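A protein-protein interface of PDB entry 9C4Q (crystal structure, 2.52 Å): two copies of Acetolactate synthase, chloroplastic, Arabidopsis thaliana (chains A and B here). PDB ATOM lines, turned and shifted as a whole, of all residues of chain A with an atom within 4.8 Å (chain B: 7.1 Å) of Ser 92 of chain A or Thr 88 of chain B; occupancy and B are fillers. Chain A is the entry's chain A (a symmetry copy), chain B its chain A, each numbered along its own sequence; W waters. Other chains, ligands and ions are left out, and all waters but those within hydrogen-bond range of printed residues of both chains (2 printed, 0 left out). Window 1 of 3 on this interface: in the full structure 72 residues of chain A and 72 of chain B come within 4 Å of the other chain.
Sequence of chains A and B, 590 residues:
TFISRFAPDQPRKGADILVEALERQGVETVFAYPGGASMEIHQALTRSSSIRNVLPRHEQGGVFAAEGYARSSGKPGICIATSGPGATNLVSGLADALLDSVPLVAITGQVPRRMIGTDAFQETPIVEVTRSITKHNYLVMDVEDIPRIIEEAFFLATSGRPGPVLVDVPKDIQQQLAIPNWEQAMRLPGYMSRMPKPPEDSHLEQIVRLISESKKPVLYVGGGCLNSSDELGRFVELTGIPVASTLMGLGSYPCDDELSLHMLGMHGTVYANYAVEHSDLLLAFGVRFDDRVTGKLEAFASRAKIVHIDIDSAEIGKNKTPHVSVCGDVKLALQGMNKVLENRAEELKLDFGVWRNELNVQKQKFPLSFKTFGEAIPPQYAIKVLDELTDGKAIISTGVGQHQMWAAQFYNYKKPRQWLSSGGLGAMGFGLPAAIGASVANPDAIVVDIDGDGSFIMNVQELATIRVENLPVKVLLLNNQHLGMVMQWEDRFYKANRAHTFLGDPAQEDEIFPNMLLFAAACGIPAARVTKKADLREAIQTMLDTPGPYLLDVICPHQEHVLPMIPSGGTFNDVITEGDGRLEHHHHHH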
ATOM      1  N   GLN A  60       8.836  18.956 -16.898  1.00  0.00           N
ATOM      2  CA  GLN A  60       9.055  18.781 -18.330  1.00  0.00           C
ATOM      3  C   GLN A  60       8.919  20.106 -19.064  1.00  0.00           C
ATOM      4  O   GLN A  60       9.640  20.359 -20.035  1.00  0.00           O
ATOM      5  CB  GLN A  60       8.090  17.748 -18.907  1.00  0.00           C
ATOM      6  CG  GLN A  60       8.175  17.641 -20.426  1.00  0.00           C
ATOM      7  CD  GLN A  60       7.524  16.386 -20.971  1.00  0.00           C
ATOM      8  OE1 GLN A  60       6.603  16.455 -21.780  1.00  0.00           O
ATOM      9  NE2 GLN A  60       8.025  15.230 -20.556  1.00  0.00           N
ATOM     10  N   PHE A  64      12.125  21.787 -21.106  1.00  0.00           N
ATOM     11  CA  PHE A  64      11.881  22.200 -22.485  1.00  0.00           C
ATOM     12  C   PHE A  64      12.045  23.706 -22.649  1.00  0.00           C
ATOM     13  O   PHE A  64      12.524  24.174 -23.689  1.00  0.00           O
ATOM     14  CB  PHE A  64      10.486  21.760 -22.925  1.00  0.00           C
ATOM     15  CG  PHE A  64      10.400  20.312 -23.311  1.00  0.00           C
ATOM     16  CD1 PHE A  64      11.546  19.581 -23.580  1.00  0.00           C
ATOM     17  CD2 PHE A  64       9.167  19.685 -23.414  1.00  0.00           C
ATOM     18  CE1 PHE A  64      11.465  18.245 -23.941  1.00  0.00           C
ATOM     19  CE2 PHE A  64       9.075  18.353 -23.773  1.00  0.00           C
ATOM     20  CZ  PHE A  64      10.226  17.629 -24.037  1.00  0.00           C
ATOM     21  N   LEU A  90      12.241  15.473 -15.619  1.00  0.00           N
ATOM     22  CA  LEU A  90      13.197  16.097 -16.524  1.00  0.00           C
ATOM     23  C   LEU A  90      13.643  15.168 -17.644  1.00  0.00           C
ATOM     24  O   LEU A  90      14.239  15.640 -18.618  1.00  0.00           O
ATOM     25  CB  LEU A  90      14.447  16.544 -15.762  1.00  0.00           C
ATOM     26  CG  LEU A  90      14.362  17.529 -14.597  1.00  0.00           C
ATOM     27  CD1 LEU A  90      15.743  17.726 -13.995  1.00  0.00           C
ATOM     28  CD2 LEU A  90      13.791  18.855 -15.057  1.00  0.00           C
ATOM     29  N   VAL A  91      13.344  13.872 -17.535  1.00  0.00           N
ATOM     30  CA  VAL A  91      14.086  12.852 -18.273  1.00  0.00           C
ATOM     31  C   VAL A  91      13.930  13.028 -19.778  1.00  0.00           C
ATOM     32  O   VAL A  91      14.901  12.893 -20.535  1.00  0.00           O
ATOM     33  CB  VAL A  91      13.651  11.447 -17.811  1.00  0.00           C
ATOM     34  CG1 VAL A  91      13.934  10.420 -18.890  1.00  0.00           C
ATOM     35  CG2 VAL A  91      14.367  11.080 -16.522  1.00  0.00           C
ATOM     36  N   SER A  92      12.711  13.322 -20.242  1.00  0.00           N
ATOM     37  CA  SER A  92      12.502  13.504 -21.676  1.00  0.00           C
ATOM     38  C   SER A  92      13.308  14.682 -22.210  1.00  0.00           C
ATOM     39  O   SER A  92      13.815  14.637 -23.338  1.00  0.00           O
ATOM     40  CB  SER A  92      11.016  13.699 -21.972  1.00  0.00           C
ATOM     41  OG  SER A  92      10.295  12.495 -21.774  1.00  0.00           O
ATOM     42  N   GLY A  93      13.442  15.742 -21.413  1.00  0.00           N
ATOM     43  CA  GLY A  93      14.211  16.892 -21.855  1.00  0.00           C
ATOM     44  C   GLY A  93      15.700  16.609 -21.931  1.00  0.00           C
ATOM     45  O   GLY A  93      16.387  17.088 -22.837  1.00  0.00           O
ATOM     46  N   LEU A  94      16.221  15.831 -20.979  1.00  0.00           N
ATOM     47  CA  LEU A  94      17.633  15.461 -21.014  1.00  0.00           C
ATOM     48  C   LEU A  94      17.951  14.647 -22.260  1.00  0.00           C
ATOM     49  O   LEU A  94      18.910  14.941 -22.982  1.00  0.00           O
ATOM     50  CB  LEU A  94      17.998  14.680 -19.749  1.00  0.00           C
ATOM     51  CG  LEU A  94      17.757  15.422 -18.436  1.00  0.00           C
ATOM     52  CD1 LEU A  94      18.070  14.521 -17.251  1.00  0.00           C
ATOM     53  CD2 LEU A  94      18.583  16.693 -18.387  1.00  0.00           C
ATOM     54  N   ALA A  95      17.146  13.616 -22.531  1.00  0.00           N
ATOM     55  CA  ALA A  95      17.332  12.820 -23.740  1.00  0.00           C
ATOM     56  C   ALA A  95      17.224  13.685 -24.990  1.00  0.00           C
ATOM     57  O   ALA A  95      18.014  13.534 -25.930  1.00  0.00           O
ATOM     58  CB  ALA A  95      16.307  11.686 -23.781  1.00  0.00           C
ATOM     59  N   ASP A  96      16.261  14.610 -25.008  1.00  0.00           N
ATOM     60  CA  ASP A  96      16.082  15.487 -26.161  1.00  0.00           C
ATOM     61  C   ASP A  96      17.294  16.389 -26.368  1.00  0.00           C
ATOM     62  O   ASP A  96      17.732  16.600 -27.504  1.00  0.00           O
ATOM     63  CB  ASP A  96      14.810  16.318 -25.982  1.00  0.00           C
ATOM     64  CG  ASP A  96      14.427  17.074 -27.236  1.00  0.00           C
ATOM     65  OD1 ASP A  96      14.407  16.452 -28.318  1.00  0.00           O
ATOM     66  OD2 ASP A  96      14.132  18.284 -27.141  1.00  0.00           O
ATOM     67  N   LEU A 425      15.074  13.204 -31.027  1.00  0.00           N
ATOM     68  CA  LEU A 425      14.109  12.464 -30.221  1.00  0.00           C
ATOM     69  C   LEU A 425      12.689  12.671 -30.731  1.00  0.00           C
ATOM     70  O   LEU A 425      11.881  11.735 -30.718  1.00  0.00           O
ATOM     71  CB  LEU A 425      14.222  12.887 -28.757  1.00  0.00           C
ATOM     72  CG  LEU A 425      13.403  12.142 -27.708  1.00  0.00           C
ATOM     73  CD1 LEU A 425      13.892  10.709 -27.570  1.00  0.00           C
ATOM     74  CD2 LEU A 425      13.476  12.873 -26.377  1.00  0.00           C
ATOM     75  N   HIS B  58      -1.233  12.084 -22.672  1.00  0.00           N
ATOM     76  CA  HIS B  58       0.173  12.161 -22.306  1.00  0.00           C
ATOM     77  C   HIS B  58       0.540  10.809 -21.713  1.00  0.00           C
ATOM     78  O   HIS B  58      -0.246  10.232 -20.958  1.00  0.00           O
ATOM     79  CB  HIS B  58       0.427  13.298 -21.304  1.00  0.00           C
ATOM     80  CG  HIS B  58       1.871  13.649 -21.122  1.00  0.00           C
ATOM     81  ND1 HIS B  58       2.812  12.740 -20.687  1.00  0.00           N
ATOM     82  CD2 HIS B  58       2.531  14.821 -21.290  1.00  0.00           C
ATOM     83  CE1 HIS B  58       3.991  13.331 -20.609  1.00  0.00           C
ATOM     84  NE2 HIS B  58       3.848  14.594 -20.968  1.00  0.00           N
ATOM     85  N   GLU B  59       1.721  10.294 -22.071  1.00  0.00           N
ATOM     86  CA  GLU B  59       2.085   8.952 -21.619  1.00  0.00           C
ATOM     87  C   GLU B  59       2.250   8.886 -20.107  1.00  0.00           C
ATOM     88  O   GLU B  59       2.029   7.826 -19.512  1.00  0.00           O
ATOM     89  CB  GLU B  59       3.361   8.472 -22.307  1.00  0.00           C
ATOM     90  CG  GLU B  59       3.199   8.203 -23.787  1.00  0.00           C
ATOM     91  CD  GLU B  59       3.527   9.410 -24.631  1.00  0.00           C
ATOM     92  OE1 GLU B  59       3.658  10.514 -24.070  1.00  0.00           O
ATOM     93  OE2 GLU B  59       3.670   9.253 -25.859  1.00  0.00           O
ATOM     94  N   GLN B  60       2.646   9.993 -19.471  1.00  0.00           N
ATOM     95  CA  GLN B  60       2.604  10.038 -18.014  1.00  0.00           C
ATOM     96  C   GLN B  60       1.182   9.855 -17.507  1.00  0.00           C
ATOM     97  O   GLN B  60       0.967   9.231 -16.461  1.00  0.00           O
ATOM     98  CB  GLN B  60       3.193  11.347 -17.490  1.00  0.00           C
ATOM     99  CG  GLN B  60       3.033  11.509 -15.984  1.00  0.00           C
ATOM    100  CD  GLN B  60       3.927  12.585 -15.402  1.00  0.00           C
ATOM    101  OE1 GLN B  60       3.449  13.541 -14.798  1.00  0.00           O
ATOM    102  NE2 GLN B  60       5.234  12.417 -15.554  1.00  0.00           N
ATOM    103  N   ALA B  81       3.560   2.567 -24.825  1.00  0.00           N
ATOM    104  CA  ALA B  81       4.066   3.801 -25.406  1.00  0.00           C
ATOM    105  C   ALA B  81       4.988   3.472 -26.569  1.00  0.00           C
ATOM    106  O   ALA B  81       5.463   2.343 -26.715  1.00  0.00           O
ATOM    107  CB  ALA B  81       4.810   4.647 -24.365  1.00  0.00           C
ATOM    108  N   THR B  82       5.237   4.475 -27.404  1.00  0.00           N
ATOM    109  CA  THR B  82       6.166   4.302 -28.507  1.00  0.00           C
ATOM    110  C   THR B  82       7.598   4.499 -28.014  1.00  0.00           C
ATOM    111  O   THR B  82       7.852   4.724 -26.827  1.00  0.00           O
ATOM    112  CB  THR B  82       5.833   5.270 -29.640  1.00  0.00           C
ATOM    113  OG1 THR B  82       6.525   4.869 -30.829  1.00  0.00           O
ATOM    114  CG2 THR B  82       6.239   6.692 -29.278  1.00  0.00           C
ATOM    115  N   SER B  83       8.550   4.422 -28.939  1.00  0.00           N
ATOM    116  CA  SER B  83       9.952   4.557 -28.578  1.00  0.00           C
ATOM    117  C   SER B  83      10.268   6.002 -28.189  1.00  0.00           C
ATOM    118  O   SER B  83       9.410   6.890 -28.211  1.00  0.00           O
ATOM    119  CB  SER B  83      10.843   4.106 -29.732  1.00  0.00           C
ATOM    120  OG  SER B  83      10.755   5.008 -30.824  1.00  0.00           O
ATOM    121  N   GLY B  84      11.527   6.224 -27.811  1.00  0.00           N
ATOM    122  CA  GLY B  84      12.054   7.547 -27.582  1.00  0.00           C
ATOM    123  C   GLY B  84      11.252   8.386 -26.606  1.00  0.00           C
ATOM    124  O   GLY B  84      11.176   8.093 -25.407  1.00  0.00           O
ATOM    125  N   PRO B  85      10.623   9.452 -27.115  1.00  0.00           N
ATOM    126  CA  PRO B  85       9.917  10.381 -26.220  1.00  0.00           C
ATOM    127  C   PRO B  85       8.685   9.781 -25.577  1.00  0.00           C
ATOM    128  O   PRO B  85       8.288  10.236 -24.496  1.00  0.00           O
ATOM    129  CB  PRO B  85       9.558  11.548 -27.146  1.00  0.00           C
ATOM    130  CG  PRO B  85       9.430  10.910 -28.491  1.00  0.00           C
ATOM    131  CD  PRO B  85      10.470   9.827 -28.531  1.00  0.00           C
ATOM    132  N   GLY B  86       8.061   8.781 -26.202  1.00  0.00           N
ATOM    133  CA  GLY B  86       6.989   8.066 -25.532  1.00  0.00           C
ATOM    134  C   GLY B  86       7.489   7.300 -24.322  1.00  0.00           C
ATOM    135  O   GLY B  86       6.916   7.391 -23.235  1.00  0.00           O
ATOM    136  N   ALA B  87       8.585   6.556 -24.492  1.00  0.00           N
ATOM    137  CA  ALA B  87       9.108   5.741 -23.402  1.00  0.00           C
ATOM    138  C   ALA B  87       9.584   6.602 -22.240  1.00  0.00           C
ATOM    139  O   ALA B  87       9.323   6.277 -21.076  1.00  0.00           O
ATOM    140  CB  ALA B  87      10.241   4.848 -23.906  1.00  0.00           C
ATOM    141  N   THR B  88      10.276   7.708 -22.533  1.00  0.00           N
ATOM    142  CA  THR B  88      10.777   8.556 -21.458  1.00  0.00           C
ATOM    143  C   THR B  88       9.645   9.211 -20.675  1.00  0.00           C
ATOM    144  O   THR B  88       9.828   9.552 -19.502  1.00  0.00           O
ATOM    145  CB  THR B  88      11.723   9.624 -22.013  1.00  0.00           C
ATOM    146  OG1 THR B  88      11.073  10.354 -23.060  1.00  0.00           O
ATOM    147  CG2 THR B  88      12.993   8.988 -22.551  1.00  0.00           C
ATOM    148  N   ASN B  89       8.472   9.386 -21.291  1.00  0.00           N
ATOM    149  CA  ASN B  89       7.336   9.949 -20.572  1.00  0.00           C
ATOM    150  C   ASN B  89       6.711   8.967 -19.587  1.00  0.00           C
ATOM    151  O   ASN B  89       5.840   9.368 -18.812  1.00  0.00           O
ATOM    152  CB  ASN B  89       6.277  10.434 -21.560  1.00  0.00           C
ATOM    153  CG  ASN B  89       6.599  11.798 -22.130  1.00  0.00           C
ATOM    154  OD1 ASN B  89       7.443  12.519 -21.600  1.00  0.00           O
ATOM    155  ND2 ASN B  89       5.917  12.165 -23.208  1.00  0.00           N
ATOM    156  N   LEU B  90       7.127   7.699 -19.598  1.00  0.00           N
ATOM    157  CA  LEU B  90       6.643   6.729 -18.626  1.00  0.00           C
ATOM    158  C   LEU B  90       7.432   6.754 -17.324  1.00  0.00           C
ATOM    159  O   LEU B  90       6.975   6.180 -16.330  1.00  0.00           O
ATOM    160  CB  LEU B  90       6.719   5.310 -19.192  1.00  0.00           C
ATOM    161  CG  LEU B  90       5.986   4.925 -20.477  1.00  0.00           C
ATOM    162  CD1 LEU B  90       6.306   3.481 -20.831  1.00  0.00           C
ATOM    163  CD2 LEU B  90       4.491   5.113 -20.319  1.00  0.00           C
ATOM    164  N   VAL B  91       8.586   7.423 -17.309  1.00  0.00           N
ATOM    165  CA  VAL B  91       9.618   7.143 -16.312  1.00  0.00           C
ATOM    166  C   VAL B  91       9.125   7.443 -14.901  1.00  0.00           C
ATOM    167  O   VAL B  91       9.386   6.675 -13.964  1.00  0.00           O
ATOM    168  CB  VAL B  91      10.901   7.926 -16.650  1.00  0.00           C
ATOM    169  CG1 VAL B  91      11.746   8.128 -15.406  1.00  0.00           C
ATOM    170  CG2 VAL B  91      11.692   7.190 -17.719  1.00  0.00           C
ATOM    171  N   SER B  92       8.417   8.560 -14.718  1.00  0.00           N
ATOM    172  CA  SER B  92       7.917   8.897 -13.388  1.00  0.00           C
ATOM    173  C   SER B  92       6.939   7.846 -12.878  1.00  0.00           C
ATOM    174  O   SER B  92       6.912   7.539 -11.681  1.00  0.00           O
ATOM    175  CB  SER B  92       7.257  10.275 -13.406  1.00  0.00           C
ATOM    176  OG  SER B  92       8.221  11.300 -13.568  1.00  0.00           O
ATOM    177  N   THR B 108       6.952  -0.845 -24.387  1.00  0.00           N
ATOM    178  CA  THR B 108       7.441   0.237 -25.230  1.00  0.00           C
ATOM    179  C   THR B 108       7.858  -0.323 -26.579  1.00  0.00           C
ATOM    180  O   THR B 108       8.543  -1.350 -26.647  1.00  0.00           O
ATOM    181  CB  THR B 108       8.624   0.967 -24.591  1.00  0.00           C
ATOM    182  OG1 THR B 108       9.575   0.012 -24.101  1.00  0.00           O
ATOM    183  CG2 THR B 108       8.161   1.855 -23.452  1.00  0.00           C
ATOM    184  N   THR B 124      15.971   5.801 -27.559  1.00  0.00           N
ATOM    185  CA  THR B 124      16.632   5.948 -26.273  1.00  0.00           C
ATOM    186  C   THR B 124      16.798   4.568 -25.658  1.00  0.00           C
ATOM    187  O   THR B 124      15.937   3.698 -25.833  1.00  0.00           O
ATOM    188  CB  THR B 124      15.850   6.850 -25.303  1.00  0.00           C
ATOM    189  OG1 THR B 124      14.485   6.428 -25.248  1.00  0.00           O
ATOM    190  CG2 THR B 124      15.929   8.295 -25.742  1.00  0.00           C
ATOM    191  N   ILE B 126      15.968   2.617 -23.285  1.00  0.00           N
ATOM    192  CA  ILE B 126      15.009   2.659 -22.185  1.00  0.00           C
ATOM    193  C   ILE B 126      15.270   1.542 -21.180  1.00  0.00           C
ATOM    194  O   ILE B 126      14.988   1.697 -19.985  1.00  0.00           O
ATOM    195  CB  ILE B 126      13.566   2.610 -22.732  1.00  0.00           C
ATOM    196  CG1 ILE B 126      12.572   3.038 -21.655  1.00  0.00           C
ATOM    197  CG2 ILE B 126      13.230   1.225 -23.267  1.00  0.00           C
ATOM    198  CD1 ILE B 126      12.791   4.449 -21.153  1.00  0.00           C
ATOM    199  N   VAL B 129      17.872   3.015 -18.995  1.00  0.00           N
ATOM    200  CA  VAL B 129      17.346   4.129 -18.211  1.00  0.00           C
ATOM    201  C   VAL B 129      16.522   3.622 -17.034  1.00  0.00           C
ATOM    202  O   VAL B 129      16.619   4.147 -15.917  1.00  0.00           O
ATOM    203  CB  VAL B 129      16.522   5.065 -19.118  1.00  0.00           C
ATOM    204  CG1 VAL B 129      15.698   6.033 -18.284  1.00  0.00           C
ATOM    205  CG2 VAL B 129      17.436   5.821 -20.069  1.00  0.00           C
ATOM    206  N   THR B 130      15.717   2.583 -17.253  1.00  0.00           N
ATOM    207  CA  THR B 130      14.727   2.148 -16.278  1.00  0.00           C
ATOM    208  C   THR B 130      15.176   0.967 -15.427  1.00  0.00           C
ATOM    209  O   THR B 130      14.371   0.458 -14.640  1.00  0.00           O
ATOM    210  CB  THR B 130      13.420   1.780 -16.986  1.00  0.00           C
ATOM    211  OG1 THR B 130      13.650   0.671 -17.864  1.00  0.00           O
ATOM    212  CG2 THR B 130      12.904   2.955 -17.796  1.00  0.00           C
HETATM  213  O   HOH W   1       6.550  14.946 -24.245  1.00  0.00           O
HETATM  214  O   HOH W   2       8.631  13.135 -24.419  1.00  0.00           O
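Ser 92 of chain A touches two residues of chain B.
Of the printed residues of chain A, Thr 88 of chain B touches Val 91 (3.9 Å) and Ser 92 (2.6 Å).
Of the printed residues of chain A, Thr 124 of chain B touches Ala 95 and Leu 425.
Printed residues of chain A within 4 Å of Asn 89 of chain B: Gln 60 (3.0 Å) and Ser 92 (2.9 Å).
Of the printed residues of chain B, Val 91 of chain A touches Thr 88.
The nearest residue of chain A that does not touch Thr 88 of chain B is Ala 95 of chain A (4.4 Å).
The nearest printed residue of chain A that does not touch Pro 85 of chain B is Ser 92 of chain A (4.1 Å).
4 positions are printed for both chains.
Of the 9 pairs that touch across the chains among the printed residues, none has its exchanged pair printed and touching as well.
Among the printed residues, pairs that only touch across the chains: Val 91 of chain A with Thr 88 of chain B (3.9 Å), Ala 95 of chain A with Thr 124 of chain B (3.9 Å), Leu 425 of chain A with Gly 84 of chain B (3.6 Å), Leu 425 of chain A with Pro 85 of chain B (3.2 Å) and Leu 425 of chain A with Thr 124 of chain B (3.6 Å).
Water W1 bridges OE1 of Gln 60 of chain A and ND2 of Asn 89 of chain B.
Water W2 lies within hydrogen-bond range of O of Pro 85 of chain B (2.9 Å), OD1 of Asn 89 of chain B (3.1 Å) and OG of Ser 92 of chain A (3.2 Å).
The side-chain amide nitrogen (NE2) of Gln 60 of chain A lies within hydrogen-bond range of the side-chain amide oxygen (OD1) of Asn 89 of chain B (3.0 Å).
The side-chain hydroxyl of Ser 92 of chain A sits at hydrogen-bond distance from the side-chain hydroxyl of Thr 88 of chain B (2.6 Å).
OE1 of Gln 60 of chain A lies within hydrogen-bond range of NE2 of His 58 of chain B (3.4 Å).
The side-chain hydroxyl (OG) of Ser 92 of chain A is in hydrogen-bond range of the side-chain amide oxygen (OD1) of Asn 89 of chain B (2.9 Å).
A ring nitrogen (ND1) of His 58 of chain B is in hydrogen-bond range of the backbone NH (N) of Gln 60 of chain B, at 3.0 Å.
The side-chain carboxylate (OE1) of Glu 59 of chain B is in hydrogen-bond range of the side-chain amide nitrogen (ND2) of Asn 89 of chain B (2.9 Å).
The backbone carbonyl oxygen of Pro 85 of chain B lies close to the side-chain amide nitrogen of Asn 89 of chain B, at 3.3 Å.
The backbone NH (N) of Gln 60 of chain B sits at hydrogen-bond distance from the backbone carbonyl oxygen (O) of Asn 89 of chain B (3.3 Å).
O of Gly 84 of chain B sits at hydrogen-bond distance from OG1 of Thr 88 of chain B (3.3 Å).
OG1 of Thr 88 of chain B is in hydrogen-bond range of O of Pro 85 of chain B, at 3.1 Å.
Of the 20 printed residues of chain B, 6 touch a printed residue of chain A.
Hydrophobic or aromatic side chains of chain B that line the printed part of chain A: His 58 and Pro 85.
Along chain B the printed residues that touch a printed residue of chain A span positions 58 to 124.
Of the 10 printed residues of chain A, 5 touch a printed residue of chain B.
Among the printed residues, no Asp or Glu carboxylate lies within 4 Å of a Lys or Arg side-chain nitrogen of the other chain.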
